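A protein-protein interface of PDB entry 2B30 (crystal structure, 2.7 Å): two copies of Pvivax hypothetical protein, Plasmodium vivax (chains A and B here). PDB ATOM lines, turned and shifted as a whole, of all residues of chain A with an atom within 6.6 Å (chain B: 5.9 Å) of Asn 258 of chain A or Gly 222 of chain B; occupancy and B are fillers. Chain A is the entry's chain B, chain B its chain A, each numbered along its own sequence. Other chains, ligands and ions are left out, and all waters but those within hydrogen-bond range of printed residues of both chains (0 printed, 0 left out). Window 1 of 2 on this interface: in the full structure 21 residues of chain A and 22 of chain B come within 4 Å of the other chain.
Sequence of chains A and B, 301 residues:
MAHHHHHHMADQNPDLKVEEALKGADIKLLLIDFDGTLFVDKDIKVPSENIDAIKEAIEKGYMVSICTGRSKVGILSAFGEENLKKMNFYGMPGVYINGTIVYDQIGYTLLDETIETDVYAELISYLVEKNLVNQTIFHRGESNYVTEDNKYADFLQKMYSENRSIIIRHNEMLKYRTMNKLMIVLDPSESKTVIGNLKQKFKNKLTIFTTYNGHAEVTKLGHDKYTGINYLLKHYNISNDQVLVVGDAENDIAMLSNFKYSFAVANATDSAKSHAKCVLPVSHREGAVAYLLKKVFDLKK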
ATOM      1  N   TYR A 226     -12.954  11.618 -22.101  1.00  0.00           N
ATOM      2  CA  TYR A 226     -11.522  11.634 -22.413  1.00  0.00           C
ATOM      3  C   TYR A 226     -11.148  10.800 -23.660  1.00  0.00           C
ATOM      4  O   TYR A 226     -10.367  11.246 -24.490  1.00  0.00           O
ATOM      5  CB  TYR A 226     -10.694  11.184 -21.198  1.00  0.00           C
ATOM      6  CG  TYR A 226      -9.207  11.277 -21.454  1.00  0.00           C
ATOM      7  CD1 TYR A 226      -8.617  12.493 -21.797  1.00  0.00           C
ATOM      8  CD2 TYR A 226      -8.384  10.150 -21.375  1.00  0.00           C
ATOM      9  CE1 TYR A 226      -7.253  12.586 -22.050  1.00  0.00           C
ATOM     10  CE2 TYR A 226      -7.016  10.242 -21.617  1.00  0.00           C
ATOM     11  CZ  TYR A 226      -6.463  11.462 -21.949  1.00  0.00           C
ATOM     12  OH  TYR A 226      -5.122  11.569 -22.200  1.00  0.00           O
ATOM     13  N   ASN A 230      -9.714  12.138 -27.471  1.00  0.00           N
ATOM     14  CA  ASN A 230      -8.545  11.645 -28.219  1.00  0.00           C
ATOM     15  C   ASN A 230      -8.778  11.508 -29.727  1.00  0.00           C
ATOM     16  O   ASN A 230      -7.872  11.745 -30.512  1.00  0.00           O
ATOM     17  CB  ASN A 230      -8.041  10.302 -27.654  1.00  0.00           C
ATOM     18  CG  ASN A 230      -7.350  10.444 -26.279  1.00  0.00           C
ATOM     19  OD1 ASN A 230      -6.963  11.547 -25.846  1.00  0.00           O
ATOM     20  ND2 ASN A 230      -7.194   9.309 -25.587  1.00  0.00           N
ATOM     21  N   ASN A 240      -1.616  17.624 -26.107  1.00  0.00           N
ATOM     22  CA  ASN A 240      -2.156  17.893 -24.770  1.00  0.00           C
ATOM     23  C   ASN A 240      -1.957  19.346 -24.343  1.00  0.00           C
ATOM     24  O   ASN A 240      -2.870  19.970 -23.817  1.00  0.00           O
ATOM     25  CB  ASN A 240      -1.522  16.946 -23.749  1.00  0.00           C
ATOM     26  CG  ASN A 240      -2.197  16.999 -22.387  1.00  0.00           C
ATOM     27  OD1 ASN A 240      -2.010  17.940 -21.621  1.00  0.00           O
ATOM     28  ND2 ASN A 240      -2.951  15.964 -22.068  1.00  0.00           N
ATOM     29  N   ILE A 253     -14.126  13.948 -14.713  1.00  0.00           N
ATOM     30  CA  ILE A 253     -12.876  13.666 -13.992  1.00  0.00           C
ATOM     31  C   ILE A 253     -11.723  13.213 -14.909  1.00  0.00           C
ATOM     32  O   ILE A 253     -10.607  13.748 -14.815  1.00  0.00           O
ATOM     33  CB  ILE A 253     -13.101  12.624 -12.869  1.00  0.00           C
ATOM     34  CG1 ILE A 253     -13.937  13.246 -11.747  1.00  0.00           C
ATOM     35  CG2 ILE A 253     -11.763  12.084 -12.339  1.00  0.00           C
ATOM     36  CD1 ILE A 253     -14.512  12.225 -10.771  1.00  0.00           C
ATOM     37  N   ALA A 254     -11.985  12.246 -15.786  1.00  0.00           N
ATOM     38  CA  ALA A 254     -10.955  11.763 -16.715  1.00  0.00           C
ATOM     39  C   ALA A 254     -10.313  12.903 -17.524  1.00  0.00           C
ATOM     40  O   ALA A 254      -9.086  12.945 -17.655  1.00  0.00           O
ATOM     41  CB  ALA A 254     -11.504  10.717 -17.638  1.00  0.00           C
ATOM     42  N   MET A 255     -11.116  13.837 -18.044  1.00  0.00           N
ATOM     43  CA  MET A 255     -10.543  14.911 -18.855  1.00  0.00           C
ATOM     44  C   MET A 255      -9.948  16.045 -17.998  1.00  0.00           C
ATOM     45  O   MET A 255      -9.093  16.784 -18.461  1.00  0.00           O
ATOM     46  CB  MET A 255     -11.545  15.428 -19.894  1.00  0.00           C
ATOM     47  CG  MET A 255     -12.597  16.370 -19.360  1.00  0.00           C
ATOM     48  SD  MET A 255     -13.767  16.907 -20.621  1.00  0.00           S
ATOM     49  CE  MET A 255     -14.786  18.006 -19.640  1.00  0.00           C
ATOM     50  N   LEU A 256     -10.383  16.172 -16.749  1.00  0.00           N
ATOM     51  CA  LEU A 256      -9.757  17.105 -15.816  1.00  0.00           C
ATOM     52  C   LEU A 256      -8.386  16.603 -15.332  1.00  0.00           C
ATOM     53  O   LEU A 256      -7.456  17.395 -15.180  1.00  0.00           O
ATOM     54  CB  LEU A 256     -10.670  17.358 -14.611  1.00  0.00           C
ATOM     55  CG  LEU A 256     -11.969  18.125 -14.876  1.00  0.00           C
ATOM     56  CD1 LEU A 256     -12.924  18.043 -13.670  1.00  0.00           C
ATOM     57  CD2 LEU A 256     -11.698  19.572 -15.227  1.00  0.00           C
ATOM     58  N   SER A 257      -8.268  15.299 -15.072  1.00  0.00           N
ATOM     59  CA  SER A 257      -6.995  14.713 -14.619  1.00  0.00           C
ATOM     60  C   SER A 257      -5.957  14.569 -15.731  1.00  0.00           C
ATOM     61  O   SER A 257      -4.765  14.498 -15.468  1.00  0.00           O
ATOM     62  CB  SER A 257      -7.211  13.319 -14.025  1.00  0.00           C
ATOM     63  OG  SER A 257      -8.201  13.330 -13.024  1.00  0.00           O
ATOM     64  N   ASN A 258      -6.413  14.498 -16.969  1.00  0.00           N
ATOM     65  CA  ASN A 258      -5.543  14.108 -18.056  1.00  0.00           C
ATOM     66  C   ASN A 258      -5.067  15.260 -18.955  1.00  0.00           C
ATOM     67  O   ASN A 258      -4.249  15.048 -19.863  1.00  0.00           O
ATOM     68  CB  ASN A 258      -6.203  12.980 -18.848  1.00  0.00           C
ATOM     69  CG  ASN A 258      -6.148  11.661 -18.106  1.00  0.00           C
ATOM     70  OD1 ASN A 258      -5.105  11.034 -18.053  1.00  0.00           O
ATOM     71  ND2 ASN A 258      -7.256  11.252 -17.506  1.00  0.00           N
ATOM     72  N   PHE A 259      -5.545  16.472 -18.688  1.00  0.00           N
ATOM     73  CA  PHE A 259      -5.007  17.653 -19.344  1.00  0.00           C
ATOM     74  C   PHE A 259      -4.418  18.573 -18.295  1.00  0.00           C
ATOM     75  O   PHE A 259      -4.802  18.506 -17.119  1.00  0.00           O
ATOM     76  CB  PHE A 259      -6.086  18.361 -20.164  1.00  0.00           C
ATOM     77  CG  PHE A 259      -6.535  17.581 -21.365  1.00  0.00           C
ATOM     78  CD1 PHE A 259      -5.724  17.483 -22.481  1.00  0.00           C
ATOM     79  CD2 PHE A 259      -7.757  16.937 -21.377  1.00  0.00           C
ATOM     80  CE1 PHE A 259      -6.120  16.751 -23.593  1.00  0.00           C
ATOM     81  CE2 PHE A 259      -8.163  16.207 -22.481  1.00  0.00           C
ATOM     82  CZ  PHE A 259      -7.335  16.111 -23.591  1.00  0.00           C
ATOM     83  N   LYS A 260      -3.479  19.419 -18.721  1.00  0.00           N
ATOM     84  CA  LYS A 260      -2.807  20.339 -17.810  1.00  0.00           C
ATOM     85  C   LYS A 260      -3.587  21.632 -17.596  1.00  0.00           C
ATOM     86  O   LYS A 260      -3.793  22.045 -16.455  1.00  0.00           O
ATOM     87  CB  LYS A 260      -1.364  20.631 -18.252  1.00  0.00           C
ATOM     88  CG  LYS A 260      -1.201  21.475 -19.495  1.00  0.00           C
ATOM     89  CD  LYS A 260       0.248  21.460 -20.006  1.00  0.00           C
ATOM     90  CE  LYS A 260       1.185  22.179 -19.062  1.00  0.00           C
ATOM     91  NZ  LYS A 260       2.553  22.164 -19.610  1.00  0.00           N
ATOM     92  N   SER A 262      -6.565  22.503 -17.208  1.00  0.00           N
ATOM     93  CA  SER A 262      -7.846  21.932 -16.839  1.00  0.00           C
ATOM     94  C   SER A 262      -8.377  22.684 -15.651  1.00  0.00           C
ATOM     95  O   SER A 262      -7.631  23.053 -14.747  1.00  0.00           O
ATOM     96  CB  SER A 262      -7.714  20.446 -16.497  1.00  0.00           C
ATOM     97  OG  SER A 262      -6.820  20.236 -15.427  1.00  0.00           O
ATOM     98  N   HIS A 275      -9.203  16.844  -8.977  1.00  0.00           N
ATOM     99  CA  HIS A 275      -8.559  16.331 -10.190  1.00  0.00           C
ATOM    100  C   HIS A 275      -8.167  17.423 -11.198  1.00  0.00           C
ATOM    101  O   HIS A 275      -7.274  17.205 -12.036  1.00  0.00           O
ATOM    102  CB  HIS A 275      -9.453  15.276 -10.835  1.00  0.00           C
ATOM    103  CG  HIS A 275      -9.484  13.984 -10.076  1.00  0.00           C
ATOM    104  ND1 HIS A 275      -8.612  12.950 -10.336  1.00  0.00           N
ATOM    105  CD2 HIS A 275     -10.256  13.573  -9.043  1.00  0.00           C
ATOM    106  CE1 HIS A 275      -8.856  11.950  -9.510  1.00  0.00           C
ATOM    107  NE2 HIS A 275      -9.847  12.303  -8.714  1.00  0.00           N
ATOM    108  N   ASN B 204      -1.354  17.569 -12.612  1.00  0.00           N
ATOM    109  CA  ASN B 204      -1.798  17.925 -13.976  1.00  0.00           C
ATOM    110  C   ASN B 204      -0.669  18.407 -14.909  1.00  0.00           C
ATOM    111  O   ASN B 204      -0.896  19.253 -15.759  1.00  0.00           O
ATOM    112  CB  ASN B 204      -2.906  18.997 -13.960  1.00  0.00           C
ATOM    113  CG  ASN B 204      -4.172  18.535 -13.274  1.00  0.00           C
ATOM    114  OD1 ASN B 204      -4.317  18.683 -12.062  1.00  0.00           O
ATOM    115  ND2 ASN B 204      -5.112  18.008 -14.048  1.00  0.00           N
ATOM    116  N   THR B 207       2.267  12.256 -15.468  1.00  0.00           N
ATOM    117  CA  THR B 207       1.764  11.019 -14.901  1.00  0.00           C
ATOM    118  C   THR B 207       2.805  10.480 -13.913  1.00  0.00           C
ATOM    119  O   THR B 207       3.947  10.202 -14.296  1.00  0.00           O
ATOM    120  CB  THR B 207       1.559  10.005 -16.029  1.00  0.00           C
ATOM    121  OG1 THR B 207       0.610  10.536 -16.957  1.00  0.00           O
ATOM    122  CG2 THR B 207       1.089   8.658 -15.505  1.00  0.00           C
ATOM    123  N   LYS B 220       4.807  11.074 -19.401  1.00  0.00           N
ATOM    124  CA  LYS B 220       4.007  12.176 -19.950  1.00  0.00           C
ATOM    125  C   LYS B 220       2.552  12.120 -19.459  1.00  0.00           C
ATOM    126  O   LYS B 220       2.009  11.038 -19.232  1.00  0.00           O
ATOM    127  CB  LYS B 220       4.043  12.120 -21.482  1.00  0.00           C
ATOM    128  CG  LYS B 220       3.454  13.345 -22.207  1.00  0.00           C
ATOM    129  CD  LYS B 220       3.456  13.128 -23.716  1.00  0.00           C
ATOM    130  CE  LYS B 220       3.324  14.428 -24.493  1.00  0.00           C
ATOM    131  NZ  LYS B 220       3.589  14.190 -25.942  1.00  0.00           N
ATOM    132  N   LEU B 221       1.936  13.290 -19.298  1.00  0.00           N
ATOM    133  CA  LEU B 221       0.553  13.392 -18.821  1.00  0.00           C
ATOM    134  C   LEU B 221      -0.415  12.859 -19.856  1.00  0.00           C
ATOM    135  O   LEU B 221      -0.193  13.012 -21.050  1.00  0.00           O
ATOM    136  CB  LEU B 221       0.201  14.852 -18.525  1.00  0.00           C
ATOM    137  CG  LEU B 221      -1.180  15.127 -17.912  1.00  0.00           C
ATOM    138  CD1 LEU B 221      -1.247  14.640 -16.483  1.00  0.00           C
ATOM    139  CD2 LEU B 221      -1.525  16.605 -17.972  1.00  0.00           C
ATOM    140  N   GLY B 222      -1.502  12.251 -19.394  1.00  0.00           N
ATOM    141  CA  GLY B 222      -2.558  11.773 -20.288  1.00  0.00           C
ATOM    142  C   GLY B 222      -2.321  10.410 -20.914  1.00  0.00           C
ATOM    143  O   GLY B 222      -3.118   9.968 -21.756  1.00  0.00           O
ATOM    144  N   HIS B 223      -1.246   9.734 -20.500  1.00  0.00           N
ATOM    145  CA  HIS B 223      -0.915   8.398 -21.010  1.00  0.00           C
ATOM    146  C   HIS B 223      -0.876   7.355 -19.906  1.00  0.00           C
ATOM    147  O   HIS B 223      -0.386   7.604 -18.808  1.00  0.00           O
ATOM    148  CB  HIS B 223       0.441   8.407 -21.735  1.00  0.00           C
ATOM    149  CG  HIS B 223       0.447   9.237 -22.977  1.00  0.00           C
ATOM    150  ND1 HIS B 223      -0.095   8.798 -24.163  1.00  0.00           N
ATOM    151  CD2 HIS B 223       0.894  10.494 -23.207  1.00  0.00           C
ATOM    152  CE1 HIS B 223       0.023   9.748 -25.074  1.00  0.00           C
ATOM    153  NE2 HIS B 223       0.622  10.785 -24.521  1.00  0.00           N
ATOM    154  N   ASP B 224      -1.405   6.180 -20.210  1.00  0.00           N
ATOM    155  CA  ASP B 224      -1.192   5.006 -19.377  1.00  0.00           C
ATOM    156  C   ASP B 224      -1.233   3.754 -20.271  1.00  0.00           C
ATOM    157  O   ASP B 224      -1.263   3.871 -21.502  1.00  0.00           O
ATOM    158  CB  ASP B 224      -2.223   4.945 -18.256  1.00  0.00           C
ATOM    159  CG  ASP B 224      -3.588   4.609 -18.763  1.00  0.00           C
ATOM    160  OD1 ASP B 224      -4.146   5.435 -19.521  1.00  0.00           O
ATOM    161  OD2 ASP B 224      -4.095   3.514 -18.421  1.00  0.00           O
ATOM    162  N   THR B 227      -4.441   3.723 -22.712  1.00  0.00           N
ATOM    163  CA  THR B 227      -4.453   4.596 -23.894  1.00  0.00           C
ATOM    164  C   THR B 227      -3.498   4.094 -24.945  1.00  0.00           C
ATOM    165  O   THR B 227      -3.761   4.255 -26.138  1.00  0.00           O
ATOM    166  CB  THR B 227      -4.040   6.028 -23.587  1.00  0.00           C
ATOM    167  OG1 THR B 227      -2.694   6.054 -23.081  1.00  0.00           O
ATOM    168  CG2 THR B 227      -4.990   6.651 -22.615  1.00  0.00           C
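Of the printed residues of chain B, Leu 256 of chain A touches Asn 204. Of the printed residues of chain B, Asn 258 of chain A touches Leu 221 and Gly 222. Of the printed residues of chain B, Phe 259 of chain A touches Asn 204 (3.1 Å) and Leu 221 (3.5 Å). Of the printed residues of chain B, Lys 260 of chain A touches Asn 204 and Leu 221. Lys 220 of chain B touches none of the printed residues of chain A. Gly 222 of chain B touches just these residues of chain A: Tyr 226 (2.6 Å) and Asn 258 (3.5 Å). The nearest printed residue of chain B that does not touch Ser 262 of chain A is Leu 221 of chain B (6.9 Å).
No position is printed for both chains. Of the 13 pairs that touch across the chains among the printed residues, none has its exchanged pair printed and touching as well.
ND2 of Asn 204 of chain B sits at hydrogen-bond distance from O of Phe 259 of chain A, at 3.1 Å. The side-chain amide nitrogen (ND2) of Asn 204 of chain B is in hydrogen-bond range of the side-chain hydroxyl (OG) of Ser 262 of chain A (3.1 Å). The side-chain amide nitrogen of Asn 204 of chain B lies within hydrogen-bond range of the backbone carbonyl oxygen of Leu 256 of chain A, at 2.7 Å. O of His 275 of chain A is in hydrogen-bond range of ND2 of Asn 204 of chain B, at 3.1 Å. The backbone carbonyl oxygen of Gly 222 of chain B is in hydrogen-bond range of the side-chain hydroxyl of Tyr 226 of chain A (2.6 Å).
The side-chain amide nitrogen (ND2) of Asn 258 of chain A lies within hydrogen-bond range of the backbone carbonyl oxygen (O) of Ala 254 of chain A (2.5 Å). ND2 of Asn 240 of chain A is in hydrogen-bond range of O of Asn 258 of chain A (2.7 Å). OG of Ser 257 of chain A lies within hydrogen-bond range of ND1 of His 275 of chain A, at 2.7 Å. The backbone carbonyl oxygen (O) of Ile 253 of chain A is in hydrogen-bond range of the side-chain hydroxyl (OG) of Ser 257 of chain A (3.0 Å). O of Phe 259 of chain A is in hydrogen-bond range of OG of Ser 262 of chain A, at 3.2 Å. The side-chain hydroxyl (OG) of Ser 262 of chain A is in hydrogen-bond range of the backbone carbonyl oxygen (O) of Leu 256 of chain A, at 2.9 Å.
Asn 240 of chain A touches Leu 221 of chain B (OD1 to CD2, 3.9 Å). Ser 257 of chain A touches Asn 204 of chain B. Leu 221 of chain B touches Ser 257 of chain A. Leu 221 of chain B touches Asn 258 of chain A. OD1 of Asn 258 of chain A touches CA of Gly 222 of chain B (3.5 Å). CD2 of Leu 221 of chain B touches C of Phe 259 of chain A (3.5 Å). CB of Lys 260 of chain A touches O of Asn 204 of chain B (2.9 Å). Lys 260 of chain A touches Leu 221 of chain B.
Of the 8 printed residues of chain B, 3 touch a printed residue of chain A. Of the 13 printed residues of chain A, 9 touch a printed residue of chain B. Among the printed residues, no Asp or Glu carboxylate lies within 4 Å of a Lys or Arg side-chain nitrogen of the other chain.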
